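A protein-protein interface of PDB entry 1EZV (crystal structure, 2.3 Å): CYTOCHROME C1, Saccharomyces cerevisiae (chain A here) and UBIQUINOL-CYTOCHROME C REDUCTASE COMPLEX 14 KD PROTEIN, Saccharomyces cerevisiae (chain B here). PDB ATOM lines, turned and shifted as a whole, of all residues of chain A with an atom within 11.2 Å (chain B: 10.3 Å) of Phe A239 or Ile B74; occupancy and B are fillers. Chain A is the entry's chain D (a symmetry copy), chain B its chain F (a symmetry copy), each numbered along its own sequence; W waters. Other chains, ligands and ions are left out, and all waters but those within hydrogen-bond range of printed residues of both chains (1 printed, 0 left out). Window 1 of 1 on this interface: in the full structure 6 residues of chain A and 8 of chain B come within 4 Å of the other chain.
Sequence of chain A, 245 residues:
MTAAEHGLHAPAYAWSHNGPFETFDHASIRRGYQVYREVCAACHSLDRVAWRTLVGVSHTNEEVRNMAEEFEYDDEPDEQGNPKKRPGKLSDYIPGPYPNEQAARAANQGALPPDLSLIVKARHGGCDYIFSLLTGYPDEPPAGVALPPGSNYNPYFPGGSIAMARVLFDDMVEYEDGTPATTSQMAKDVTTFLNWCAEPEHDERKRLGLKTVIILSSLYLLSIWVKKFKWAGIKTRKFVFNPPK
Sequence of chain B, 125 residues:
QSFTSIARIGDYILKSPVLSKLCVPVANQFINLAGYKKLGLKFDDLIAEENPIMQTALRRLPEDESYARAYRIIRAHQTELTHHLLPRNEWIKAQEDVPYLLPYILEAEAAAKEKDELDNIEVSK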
ATOM      1  N   ALA A 232     -36.893   2.132  21.124  1.00  0.00           N
ATOM      2  CA  ALA A 232     -36.546   0.726  21.391  1.00  0.00           C
ATOM      3  C   ALA A 232     -35.166   0.322  20.872  1.00  0.00           C
ATOM      4  O   ALA A 232     -34.442  -0.416  21.538  1.00  0.00           O
ATOM      5  CB  ALA A 232     -37.618  -0.218  20.828  1.00  0.00           C
ATOM      6  N   GLY A 233     -34.770   0.858  19.726  1.00  0.00           N
ATOM      7  CA  GLY A 233     -33.430   0.607  19.232  1.00  0.00           C
ATOM      8  C   GLY A 233     -32.339   1.115  20.158  1.00  0.00           C
ATOM      9  O   GLY A 233     -31.303   0.463  20.318  1.00  0.00           O
ATOM     10  N   ILE A 234     -32.571   2.274  20.773  1.00  0.00           N
ATOM     11  CA  ILE A 234     -31.566   2.926  21.619  1.00  0.00           C
ATOM     12  C   ILE A 234     -31.515   2.288  23.011  1.00  0.00           C
ATOM     13  O   ILE A 234     -30.438   1.992  23.530  1.00  0.00           O
ATOM     14  CB  ILE A 234     -31.848   4.465  21.733  1.00  0.00           C
ATOM     15  CG1 ILE A 234     -31.564   5.144  20.389  1.00  0.00           C
ATOM     16  CG2 ILE A 234     -31.000   5.105  22.835  1.00  0.00           C
ATOM     17  CD1 ILE A 234     -30.124   5.023  19.913  1.00  0.00           C
ATOM     18  N   LYS A 235     -32.683   1.935  23.536  1.00  0.00           N
ATOM     19  CA  LYS A 235     -32.773   1.382  24.876  1.00  0.00           C
ATOM     20  C   LYS A 235     -32.161  -0.011  24.991  1.00  0.00           C
ATOM     21  O   LYS A 235     -31.587  -0.353  26.025  1.00  0.00           O
ATOM     22  CB  LYS A 235     -34.229   1.348  25.333  1.00  0.00           C
ATOM     23  CG  LYS A 235     -34.804   2.717  25.627  1.00  0.00           C
ATOM     24  CD  LYS A 235     -34.742   3.042  27.109  1.00  0.00           C
ATOM     25  CE  LYS A 235     -35.181   4.474  27.374  1.00  0.00           C
ATOM     26  NZ  LYS A 235     -35.415   4.737  28.817  1.00  0.00           N
ATOM     27  N   THR A 236     -32.278  -0.811  23.936  1.00  0.00           N
ATOM     28  CA  THR A 236     -31.760  -2.176  23.973  1.00  0.00           C
ATOM     29  C   THR A 236     -30.415  -2.316  23.264  1.00  0.00           C
ATOM     30  O   THR A 236     -29.867  -3.402  23.168  1.00  0.00           O
ATOM     31  CB  THR A 236     -32.776  -3.173  23.380  1.00  0.00           C
ATOM     32  OG1 THR A 236     -33.122  -2.772  22.049  1.00  0.00           O
ATOM     33  CG2 THR A 236     -34.041  -3.214  24.247  1.00  0.00           C
ATOM     34  N   ARG A 237     -29.855  -1.186  22.854  1.00  0.00           N
ATOM     35  CA  ARG A 237     -28.523  -1.105  22.262  1.00  0.00           C
ATOM     36  C   ARG A 237     -27.488  -1.753  23.193  1.00  0.00           C
ATOM     37  O   ARG A 237     -27.611  -1.659  24.414  1.00  0.00           O
ATOM     38  CB  ARG A 237     -28.193   0.375  22.040  1.00  0.00           C
ATOM     39  CG  ARG A 237     -26.943   0.679  21.257  1.00  0.00           C
ATOM     40  CD  ARG A 237     -26.919   2.161  20.874  1.00  0.00           C
ATOM     41  NE  ARG A 237     -27.179   3.045  22.013  1.00  0.00           N
ATOM     42  CZ  ARG A 237     -26.643   4.256  22.167  1.00  0.00           C
ATOM     43  NH1 ARG A 237     -26.835   4.929  23.295  1.00  0.00           N
ATOM     44  NH2 ARG A 237     -25.960   4.822  21.179  1.00  0.00           N
ATOM     45  N   LYS A 238     -26.515  -2.459  22.612  1.00  0.00           N
ATOM     46  CA  LYS A 238     -25.464  -3.124  23.390  1.00  0.00           C
ATOM     47  C   LYS A 238     -24.072  -2.773  22.888  1.00  0.00           C
ATOM     48  O   LYS A 238     -23.828  -2.754  21.682  1.00  0.00           O
ATOM     49  CB  LYS A 238     -25.634  -4.645  23.343  1.00  0.00           C
ATOM     50  CG  LYS A 238     -27.061  -5.110  23.531  1.00  0.00           C
ATOM     51  CD  LYS A 238     -27.168  -6.216  24.558  1.00  0.00           C
ATOM     52  CE  LYS A 238     -28.626  -6.588  24.798  1.00  0.00           C
ATOM     53  NZ  LYS A 238     -28.769  -7.901  25.502  1.00  0.00           N
ATOM     54  N   PHE A 239     -23.149  -2.563  23.821  1.00  0.00           N
ATOM     55  CA  PHE A 239     -21.761  -2.246  23.486  1.00  0.00           C
ATOM     56  C   PHE A 239     -20.795  -3.389  23.873  1.00  0.00           C
ATOM     57  O   PHE A 239     -21.074  -4.172  24.791  1.00  0.00           O
ATOM     58  CB  PHE A 239     -21.336  -0.948  24.186  1.00  0.00           C
ATOM     59  CG  PHE A 239     -22.017   0.287  23.659  1.00  0.00           C
ATOM     60  CD1 PHE A 239     -23.286   0.652  24.115  1.00  0.00           C
ATOM     61  CD2 PHE A 239     -21.403   1.079  22.694  1.00  0.00           C
ATOM     62  CE1 PHE A 239     -23.937   1.786  23.613  1.00  0.00           C
ATOM     63  CE2 PHE A 239     -22.043   2.214  22.182  1.00  0.00           C
ATOM     64  CZ  PHE A 239     -23.316   2.564  22.644  1.00  0.00           C
ATOM     65  N   VAL A 240     -19.718  -3.543  23.100  1.00  0.00           N
ATOM     66  CA  VAL A 240     -18.586  -4.379  23.499  1.00  0.00           C
ATOM     67  C   VAL A 240     -17.257  -3.647  23.307  1.00  0.00           C
ATOM     68  O   VAL A 240     -17.050  -2.962  22.311  1.00  0.00           O
ATOM     69  CB  VAL A 240     -18.525  -5.707  22.702  1.00  0.00           C
ATOM     70  CG1 VAL A 240     -19.719  -6.570  23.023  1.00  0.00           C
ATOM     71  CG2 VAL A 240     -18.449  -5.427  21.213  1.00  0.00           C
ATOM     72  N   PHE A 241     -16.348  -3.822  24.256  1.00  0.00           N
ATOM     73  CA  PHE A 241     -15.026  -3.218  24.167  1.00  0.00           C
ATOM     74  C   PHE A 241     -13.957  -4.300  23.962  1.00  0.00           C
ATOM     75  O   PHE A 241     -13.940  -5.313  24.663  1.00  0.00           O
ATOM     76  CB  PHE A 241     -14.745  -2.423  25.442  1.00  0.00           C
ATOM     77  CG  PHE A 241     -13.439  -1.678  25.432  1.00  0.00           C
ATOM     78  CD1 PHE A 241     -13.073  -0.888  24.341  1.00  0.00           C
ATOM     79  CD2 PHE A 241     -12.608  -1.703  26.548  1.00  0.00           C
ATOM     80  CE1 PHE A 241     -11.904  -0.127  24.361  1.00  0.00           C
ATOM     81  CE2 PHE A 241     -11.430  -0.944  26.580  1.00  0.00           C
ATOM     82  CZ  PHE A 241     -11.081  -0.153  25.482  1.00  0.00           C
ATOM     83  N   ASN A 242     -13.161  -4.135  22.910  1.00  0.00           N
ATOM     84  CA  ASN A 242     -11.980  -4.959  22.689  1.00  0.00           C
ATOM     85  C   ASN A 242     -10.767  -4.039  22.637  1.00  0.00           C
ATOM     86  O   ASN A 242     -10.552  -3.343  21.647  1.00  0.00           O
ATOM     87  CB  ASN A 242     -12.104  -5.741  21.375  1.00  0.00           C
ATOM     88  CG  ASN A 242     -13.159  -6.825  21.441  1.00  0.00           C
ATOM     89  OD1 ASN A 242     -13.195  -7.611  22.383  1.00  0.00           O
ATOM     90  ND2 ASN A 242     -14.033  -6.865  20.448  1.00  0.00           N
ATOM     91  N   PRO A 243     -10.022  -3.943  23.748  1.00  0.00           N
ATOM     92  CA  PRO A 243      -8.968  -2.928  23.831  1.00  0.00           C
ATOM     93  C   PRO A 243      -7.914  -3.067  22.730  1.00  0.00           C
ATOM     94  O   PRO A 243      -7.462  -4.171  22.421  1.00  0.00           O
ATOM     95  CB  PRO A 243      -8.384  -3.120  25.237  1.00  0.00           C
ATOM     96  CG  PRO A 243      -9.032  -4.361  25.786  1.00  0.00           C
ATOM     97  CD  PRO A 243     -10.311  -4.541  25.059  1.00  0.00           C
ATOM     98  N   LEU B  39     -22.030   2.006  38.063  1.00  0.00           N
ATOM     99  CA  LEU B  39     -22.214   2.377  36.661  1.00  0.00           C
ATOM    100  C   LEU B  39     -20.980   2.037  35.824  1.00  0.00           C
ATOM    101  O   LEU B  39     -20.969   2.247  34.603  1.00  0.00           O
ATOM    102  CB  LEU B  39     -22.496   3.878  36.545  1.00  0.00           C
ATOM    103  CG  LEU B  39     -23.940   4.344  36.370  1.00  0.00           C
ATOM    104  CD1 LEU B  39     -24.905   3.416  37.071  1.00  0.00           C
ATOM    105  CD2 LEU B  39     -24.064   5.751  36.920  1.00  0.00           C
ATOM    106  N   GLY B  40     -19.915   1.603  36.493  1.00  0.00           N
ATOM    107  CA  GLY B  40     -18.714   1.197  35.790  1.00  0.00           C
ATOM    108  C   GLY B  40     -17.723   2.327  35.629  1.00  0.00           C
ATOM    109  O   GLY B  40     -16.822   2.257  34.793  1.00  0.00           O
ATOM    110  N   LEU B  41     -17.864   3.353  36.456  1.00  0.00           N
ATOM    111  CA  LEU B  41     -16.994   4.520  36.382  1.00  0.00           C
ATOM    112  C   LEU B  41     -15.918   4.495  37.450  1.00  0.00           C
ATOM    113  O   LEU B  41     -16.066   3.856  38.494  1.00  0.00           O
ATOM    114  CB  LEU B  41     -17.810   5.815  36.517  1.00  0.00           C
ATOM    115  CG  LEU B  41     -18.760   6.121  35.357  1.00  0.00           C
ATOM    116  CD1 LEU B  41     -19.780   7.178  35.768  1.00  0.00           C
ATOM    117  CD2 LEU B  41     -17.962   6.579  34.159  1.00  0.00           C
ATOM    118  N   ASP B  45     -13.027   9.624  36.018  1.00  0.00           N
ATOM    119  CA  ASP B  45     -13.934   9.778  34.871  1.00  0.00           C
ATOM    120  C   ASP B  45     -14.982  10.865  35.109  1.00  0.00           C
ATOM    121  O   ASP B  45     -15.606  11.339  34.168  1.00  0.00           O
ATOM    122  CB  ASP B  45     -14.678   8.475  34.561  1.00  0.00           C
ATOM    123  CG  ASP B  45     -13.753   7.297  34.338  1.00  0.00           C
ATOM    124  OD1 ASP B  45     -12.630   7.477  33.842  1.00  0.00           O
ATOM    125  OD2 ASP B  45     -14.192   6.163  34.586  1.00  0.00           O
ATOM    126  N   LEU B  46     -15.222  11.182  36.380  1.00  0.00           N
ATOM    127  CA  LEU B  46     -16.265  12.112  36.803  1.00  0.00           C
ATOM    128  C   LEU B  46     -15.844  13.579  36.819  1.00  0.00           C
ATOM    129  O   LEU B  46     -16.673  14.452  37.061  1.00  0.00           O
ATOM    130  CB  LEU B  46     -16.738  11.744  38.206  1.00  0.00           C
ATOM    131  CG  LEU B  46     -17.938  10.819  38.355  1.00  0.00           C
ATOM    132  CD1 LEU B  46     -18.038   9.873  37.166  1.00  0.00           C
ATOM    133  CD2 LEU B  46     -17.806  10.062  39.667  1.00  0.00           C
ATOM    134  N   SER B  66      -6.950   6.303  27.416  1.00  0.00           N
ATOM    135  CA  SER B  66      -7.914   7.154  26.730  1.00  0.00           C
ATOM    136  C   SER B  66      -9.076   6.373  26.119  1.00  0.00           C
ATOM    137  O   SER B  66     -10.239   6.735  26.309  1.00  0.00           O
ATOM    138  CB  SER B  66      -7.228   7.971  25.651  1.00  0.00           C
ATOM    139  OG  SER B  66      -8.148   8.884  25.091  1.00  0.00           O
ATOM    140  N   TYR B  67      -8.764   5.277  25.433  1.00  0.00           N
ATOM    141  CA  TYR B  67      -9.805   4.433  24.844  1.00  0.00           C
ATOM    142  C   TYR B  67     -10.656   3.796  25.938  1.00  0.00           C
ATOM    143  O   TYR B  67     -11.857   3.592  25.760  1.00  0.00           O
ATOM    144  CB  TYR B  67      -9.192   3.325  23.972  1.00  0.00           C
ATOM    145  CG  TYR B  67      -8.356   3.804  22.800  1.00  0.00           C
ATOM    146  CD1 TYR B  67      -7.204   3.114  22.419  1.00  0.00           C
ATOM    147  CD2 TYR B  67      -8.731   4.927  22.048  1.00  0.00           C
ATOM    148  CE1 TYR B  67      -6.451   3.522  21.321  1.00  0.00           C
ATOM    149  CE2 TYR B  67      -7.981   5.345  20.952  1.00  0.00           C
ATOM    150  CZ  TYR B  67      -6.843   4.635  20.592  1.00  0.00           C
ATOM    151  OH  TYR B  67      -6.103   5.025  19.497  1.00  0.00           O
ATOM    152  N   ALA B  68     -10.023   3.481  27.067  1.00  0.00           N
ATOM    153  CA  ALA B  68     -10.716   2.857  28.190  1.00  0.00           C
ATOM    154  C   ALA B  68     -11.691   3.824  28.878  1.00  0.00           C
ATOM    155  O   ALA B  68     -12.836   3.455  29.157  1.00  0.00           O
ATOM    156  CB  ALA B  68      -9.699   2.314  29.199  1.00  0.00           C
ATOM    157  N   ARG B  69     -11.243   5.061  29.116  1.00  0.00           N
ATOM    158  CA  ARG B  69     -12.118   6.112  29.638  1.00  0.00           C
ATOM    159  C   ARG B  69     -13.331   6.311  28.728  1.00  0.00           C
ATOM    160  O   ARG B  69     -14.469   6.346  29.205  1.00  0.00           O
ATOM    161  CB  ARG B  69     -11.366   7.449  29.802  1.00  0.00           C
ATOM    162  CG  ARG B  69     -12.180   8.486  30.579  1.00  0.00           C
ATOM    163  CD  ARG B  69     -11.498   9.843  30.723  1.00  0.00           C
ATOM    164  NE  ARG B  69     -11.587  10.570  29.474  1.00  0.00           N
ATOM    165  CZ  ARG B  69     -12.444  11.545  29.210  1.00  0.00           C
ATOM    166  NH1 ARG B  69     -12.678  11.829  27.943  1.00  0.00           N
ATOM    167  NH2 ARG B  69     -12.853  12.390  30.161  1.00  0.00           N
ATOM    168  N   ALA B  70     -13.093   6.284  27.418  1.00  0.00           N
ATOM    169  CA  ALA B  70     -14.151   6.483  26.427  1.00  0.00           C
ATOM    170  C   ALA B  70     -15.222   5.399  26.520  1.00  0.00           C
ATOM    171  O   ALA B  70     -16.422   5.693  26.510  1.00  0.00           O
ATOM    172  CB  ALA B  70     -13.556   6.516  25.017  1.00  0.00           C
ATOM    173  N   TYR B  71     -14.784   4.152  26.665  1.00  0.00           N
ATOM    174  CA  TYR B  71     -15.708   3.033  26.828  1.00  0.00           C
ATOM    175  C   TYR B  71     -16.500   3.124  28.132  1.00  0.00           C
ATOM    176  O   TYR B  71     -17.701   2.852  28.149  1.00  0.00           O
ATOM    177  CB  TYR B  71     -14.952   1.693  26.774  1.00  0.00           C
ATOM    178  CG  TYR B  71     -15.843   0.493  26.985  1.00  0.00           C
ATOM    179  CD1 TYR B  71     -16.904   0.235  26.121  1.00  0.00           C
ATOM    180  CD2 TYR B  71     -15.699  -0.320  28.112  1.00  0.00           C
ATOM    181  CE1 TYR B  71     -17.811  -0.795  26.374  1.00  0.00           C
ATOM    182  CE2 TYR B  71     -16.606  -1.354  28.378  1.00  0.00           C
ATOM    183  CZ  TYR B  71     -17.658  -1.584  27.504  1.00  0.00           C
ATOM    184  OH  TYR B  71     -18.563  -2.597  27.752  1.00  0.00           O
ATOM    185  N   ARG B  72     -15.822   3.463  29.225  1.00  0.00           N
ATOM    186  CA  ARG B  72     -16.475   3.529  30.529  1.00  0.00           C
ATOM    187  C   ARG B  72     -17.543   4.617  30.559  1.00  0.00           C
ATOM    188  O   ARG B  72     -18.652   4.396  31.055  1.00  0.00           O
ATOM    189  CB  ARG B  72     -15.447   3.771  31.641  1.00  0.00           C
ATOM    190  CG  ARG B  72     -14.571   2.568  31.954  1.00  0.00           C
ATOM    191  CD  ARG B  72     -13.846   2.729  33.283  1.00  0.00           C
ATOM    192  NE  ARG B  72     -13.025   3.942  33.342  1.00  0.00           N
ATOM    193  CZ  ARG B  72     -11.761   4.025  32.935  1.00  0.00           C
ATOM    194  NH1 ARG B  72     -11.110   5.178  33.028  1.00  0.00           N
ATOM    195  NH2 ARG B  72     -11.154   2.972  32.410  1.00  0.00           N
ATOM    196  N   ILE B  73     -17.245   5.747  29.923  1.00  0.00           N
ATOM    197  CA  ILE B  73     -18.194   6.853  29.817  1.00  0.00           C
ATOM    198  C   ILE B  73     -19.410   6.510  28.938  1.00  0.00           C
ATOM    199  O   ILE B  73     -20.567   6.712  29.342  1.00  0.00           O
ATOM    200  CB  ILE B  73     -17.482   8.118  29.290  1.00  0.00           C
ATOM    201  CG1 ILE B  73     -16.520   8.641  30.366  1.00  0.00           C
ATOM    202  CG2 ILE B  73     -18.505   9.198  28.919  1.00  0.00           C
ATOM    203  CD1 ILE B  73     -15.595   9.748  29.898  1.00  0.00           C
ATOM    204  N   ILE B  74     -19.158   5.897  27.787  1.00  0.00           N
ATOM    205  CA  ILE B  74     -20.253   5.494  26.911  1.00  0.00           C
ATOM    206  C   ILE B  74     -21.123   4.437  27.580  1.00  0.00           C
ATOM    207  O   ILE B  74     -22.346   4.572  27.632  1.00  0.00           O
ATOM    208  CB  ILE B  74     -19.733   4.969  25.558  1.00  0.00           C
ATOM    209  CG1 ILE B  74     -19.076   6.110  24.782  1.00  0.00           C
ATOM    210  CG2 ILE B  74     -20.872   4.388  24.747  1.00  0.00           C
ATOM    211  CD1 ILE B  74     -18.402   5.677  23.498  1.00  0.00           C
ATOM    212  N   ARG B  75     -20.482   3.475  28.229  1.00  0.00           N
ATOM    213  CA  ARG B  75     -21.205   2.418  28.945  1.00  0.00           C
ATOM    214  C   ARG B  75     -22.035   2.971  30.113  1.00  0.00           C
ATOM    215  O   ARG B  75     -23.168   2.541  30.334  1.00  0.00           O
ATOM    216  CB  ARG B  75     -20.211   1.359  29.441  1.00  0.00           C
ATOM    217  CG  ARG B  75     -20.826   0.182  30.162  1.00  0.00           C
ATOM    218  CD  ARG B  75     -20.076  -0.063  31.455  1.00  0.00           C
ATOM    219  NE  ARG B  75     -19.025  -1.067  31.320  1.00  0.00           N
ATOM    220  CZ  ARG B  75     -17.915  -1.113  32.049  1.00  0.00           C
ATOM    221  NH1 ARG B  75     -17.127  -2.172  31.953  1.00  0.00           N
ATOM    222  NH2 ARG B  75     -17.522  -0.068  32.766  1.00  0.00           N
ATOM    223  N   ALA B  76     -21.511   3.993  30.786  1.00  0.00           N
ATOM    224  CA  ALA B  76     -22.252   4.659  31.854  1.00  0.00           C
ATOM    225  C   ALA B  76     -23.515   5.375  31.345  1.00  0.00           C
ATOM    226  O   ALA B  76     -24.580   5.278  31.968  1.00  0.00           O
ATOM    227  CB  ALA B  76     -21.343   5.645  32.586  1.00  0.00           C
ATOM    228  N   HIS B  77     -23.411   6.068  30.208  1.00  0.00           N
ATOM    229  CA  HIS B  77     -24.573   6.755  29.641  1.00  0.00           C
ATOM    230  C   HIS B  77     -25.671   5.794  29.215  1.00  0.00           C
ATOM    231  O   HIS B  77     -26.851   6.034  29.499  1.00  0.00           O
ATOM    232  CB  HIS B  77     -24.168   7.636  28.456  1.00  0.00           C
ATOM    233  CG  HIS B  77     -23.578   8.950  28.862  1.00  0.00           C
ATOM    234  ND1 HIS B  77     -22.260   9.280  28.628  1.00  0.00           N
ATOM    235  CD2 HIS B  77     -24.135  10.031  29.456  1.00  0.00           C
ATOM    236  CE1 HIS B  77     -22.035  10.513  29.045  1.00  0.00           C
ATOM    237  NE2 HIS B  77     -23.159  10.991  29.551  1.00  0.00           N
ATOM    238  N   GLN B  78     -25.277   4.699  28.566  1.00  0.00           N
ATOM    239  CA  GLN B  78     -26.221   3.675  28.133  1.00  0.00           C
ATOM    240  C   GLN B  78     -26.935   3.015  29.307  1.00  0.00           C
ATOM    241  O   GLN B  78     -28.144   2.784  29.252  1.00  0.00           O
ATOM    242  CB  GLN B  78     -25.514   2.602  27.307  1.00  0.00           C
ATOM    243  CG  GLN B  78     -26.444   1.487  26.845  1.00  0.00           C
ATOM    244  CD  GLN B  78     -27.533   1.984  25.907  1.00  0.00           C
ATOM    245  OE1 GLN B  78     -27.321   2.917  25.128  1.00  0.00           O
ATOM    246  NE2 GLN B  78     -28.705   1.367  25.980  1.00  0.00           N
ATOM    247  N   THR B  79     -26.201   2.733  30.380  1.00  0.00           N
ATOM    248  CA  THR B  79     -26.821   2.139  31.558  1.00  0.00           C
ATOM    249  C   THR B  79     -27.735   3.145  32.258  1.00  0.00           C
ATOM    250  O   THR B  79     -28.858   2.814  32.633  1.00  0.00           O
ATOM    251  CB  THR B  79     -25.762   1.621  32.558  1.00  0.00           C
ATOM    252  OG1 THR B  79     -24.753   0.895  31.849  1.00  0.00           O
ATOM    253  CG2 THR B  79     -26.408   0.694  33.576  1.00  0.00           C
ATOM    254  N   GLU B  80     -27.274   4.383  32.389  1.00  0.00           N
ATOM    255  CA  GLU B  80     -28.107   5.436  32.955  1.00  0.00           C
ATOM    256  C   GLU B  80     -29.450   5.548  32.227  1.00  0.00           C
ATOM    257  O   GLU B  80     -30.502   5.557  32.866  1.00  0.00           O
ATOM    258  CB  GLU B  80     -27.372   6.780  32.909  1.00  0.00           C
ATOM    259  CG  GLU B  80     -28.125   7.940  33.555  1.00  0.00           C
ATOM    260  CD  GLU B  80     -28.570   7.649  34.979  1.00  0.00           C
ATOM    261  OE1 GLU B  80     -29.711   7.998  35.323  1.00  0.00           O
ATOM    262  OE2 GLU B  80     -27.785   7.079  35.763  1.00  0.00           O
ATOM    263  N   LEU B  81     -29.420   5.544  30.895  1.00  0.00           N
ATOM    264  CA  LEU B  81     -30.652   5.720  30.127  1.00  0.00           C
ATOM    265  C   LEU B  81     -31.592   4.518  30.180  1.00  0.00           C
ATOM    266  O   LEU B  81     -32.772   4.648  29.874  1.00  0.00           O
ATOM    267  CB  LEU B  81     -30.351   6.101  28.667  1.00  0.00           C
ATOM    268  CG  LEU B  81     -29.889   5.080  27.621  1.00  0.00           C
ATOM    269  CD1 LEU B  81     -31.051   4.294  27.051  1.00  0.00           C
ATOM    270  CD2 LEU B  81     -29.190   5.835  26.512  1.00  0.00           C
ATOM    271  N   THR B  82     -31.082   3.356  30.577  1.00  0.00           N
ATOM    272  CA  THR B  82     -31.948   2.189  30.739  1.00  0.00           C
ATOM    273  C   THR B  82     -32.464   2.066  32.165  1.00  0.00           C
ATOM    274  O   THR B  82     -33.228   1.155  32.464  1.00  0.00           O
ATOM    275  CB  THR B  82     -31.233   0.874  30.362  1.00  0.00           C
ATOM    276  OG1 THR B  82     -30.075   0.699  31.186  1.00  0.00           O
ATOM    277  CG2 THR B  82     -30.811   0.898  28.917  1.00  0.00           C
ATOM    278  N   LEU B  86     -25.148  -1.821  36.285  1.00  0.00           N
ATOM    279  CA  LEU B  86     -24.494  -2.956  35.662  1.00  0.00           C
ATOM    280  C   LEU B  86     -24.655  -4.196  36.548  1.00  0.00           C
ATOM    281  O   LEU B  86     -24.951  -4.082  37.737  1.00  0.00           O
ATOM    282  CB  LEU B  86     -23.016  -2.639  35.444  1.00  0.00           C
ATOM    283  CG  LEU B  86     -22.725  -1.510  34.452  1.00  0.00           C
ATOM    284  CD1 LEU B  86     -21.238  -1.193  34.464  1.00  0.00           C
ATOM    285  CD2 LEU B  86     -23.177  -1.917  33.057  1.00  0.00           C
ATOM    286  N   GLU B  90     -19.466  -6.573  36.966  1.00  0.00           N
ATOM    287  CA  GLU B  90     -18.936  -5.553  36.067  1.00  0.00           C
ATOM    288  C   GLU B  90     -18.596  -4.242  36.777  1.00  0.00           C
ATOM    289  O   GLU B  90     -17.998  -3.349  36.174  1.00  0.00           O
ATOM    290  CB  GLU B  90     -19.929  -5.271  34.938  1.00  0.00           C
ATOM    291  CG  GLU B  90     -19.881  -6.253  33.779  1.00  0.00           C
ATOM    292  CD  GLU B  90     -20.888  -5.906  32.698  1.00  0.00           C
ATOM    293  OE1 GLU B  90     -20.649  -4.926  31.953  1.00  0.00           O
ATOM    294  OE2 GLU B  90     -21.933  -6.588  32.617  1.00  0.00           O
HETATM  295  O   HOH W   1     -33.859   7.502  28.781  1.00  0.00           O
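O of Lys A235 is in hydrogen-bond range of NE2 of Gln B78. The guanidinium group of Arg A237 sits at hydrogen-bond distance from the side-chain amide oxygen of Gln B78, 2.8 Å away. The backbone carbonyl oxygen (O) of Ile A234 lies within hydrogen-bond range of the side-chain amide nitrogen (NE2) of Gln B78 (3.1 Å). The backbone carbonyl oxygen (O) of Leu B81 sits at hydrogen-bond distance from the side-chain amino group (NZ) of Lys A235.
The backbone carbonyl oxygen (O) of Gln B78 sits close to the side-chain hydroxyl (OG1) of Thr B82 (3.4 Å). The backbone carbonyl oxygen (O) of Thr B79 lies within hydrogen-bond range of the side-chain hydroxyl (OG1) of Thr B82, at 2.8 Å.
CG2 of Thr B82 touches O of Lys A235, 3.2 Å away. Phe A239 touches Ile B74 (CE2 to CG2, 3.6 Å). Phe A239 touches Gln B78 (CE1 to OE1, 3.9 Å). Phe A241 touches Tyr B67 (CZ to O, 3.8 Å). Tyr B71 touches Phe A241.
Of the printed residues of chain B, Ile A234 touches Gln B78 (3.1 Å). Of the printed residues of chain B, Phe A239 touches Ile B74 and Gln B78. Val A240 touches none of the printed residues of chain B. No residue of chain A comes within 4 Å of Ala B70. Tyr B71 touches one residue of chain A. No residue of chain A comes within 4 Å of Ile B73. Ala B76 touches none of the printed residues of chain A. No residue of chain A comes within 4 Å of His B77. Of the printed residues of chain A, Thr B82 touches Lys A235.
Of the 24 printed residues of chain B, 6 touch a printed residue of chain A. Printed residues of chain B that touch a printed residue of chain A: Tyr B67, Tyr B71, Ile B74, Gln B78, Leu B81 and Thr B82. Hydrophobic or aromatic side chains of chain B within 4 Å of the printed part of chain A: Tyr B71, Ile B74 and Leu B81. Among the printed residues, 9 pairs touch across the chains. Among the printed residues, no Asp or Glu carboxylate lies within 4 Å of a Lys or Arg side-chain nitrogen of the other chain.
Water W1 bridges the side-chain amino group of Lys A235 (3.2 Å) and the backbone carbonyl oxygen of Leu B81 (3.2 Å).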
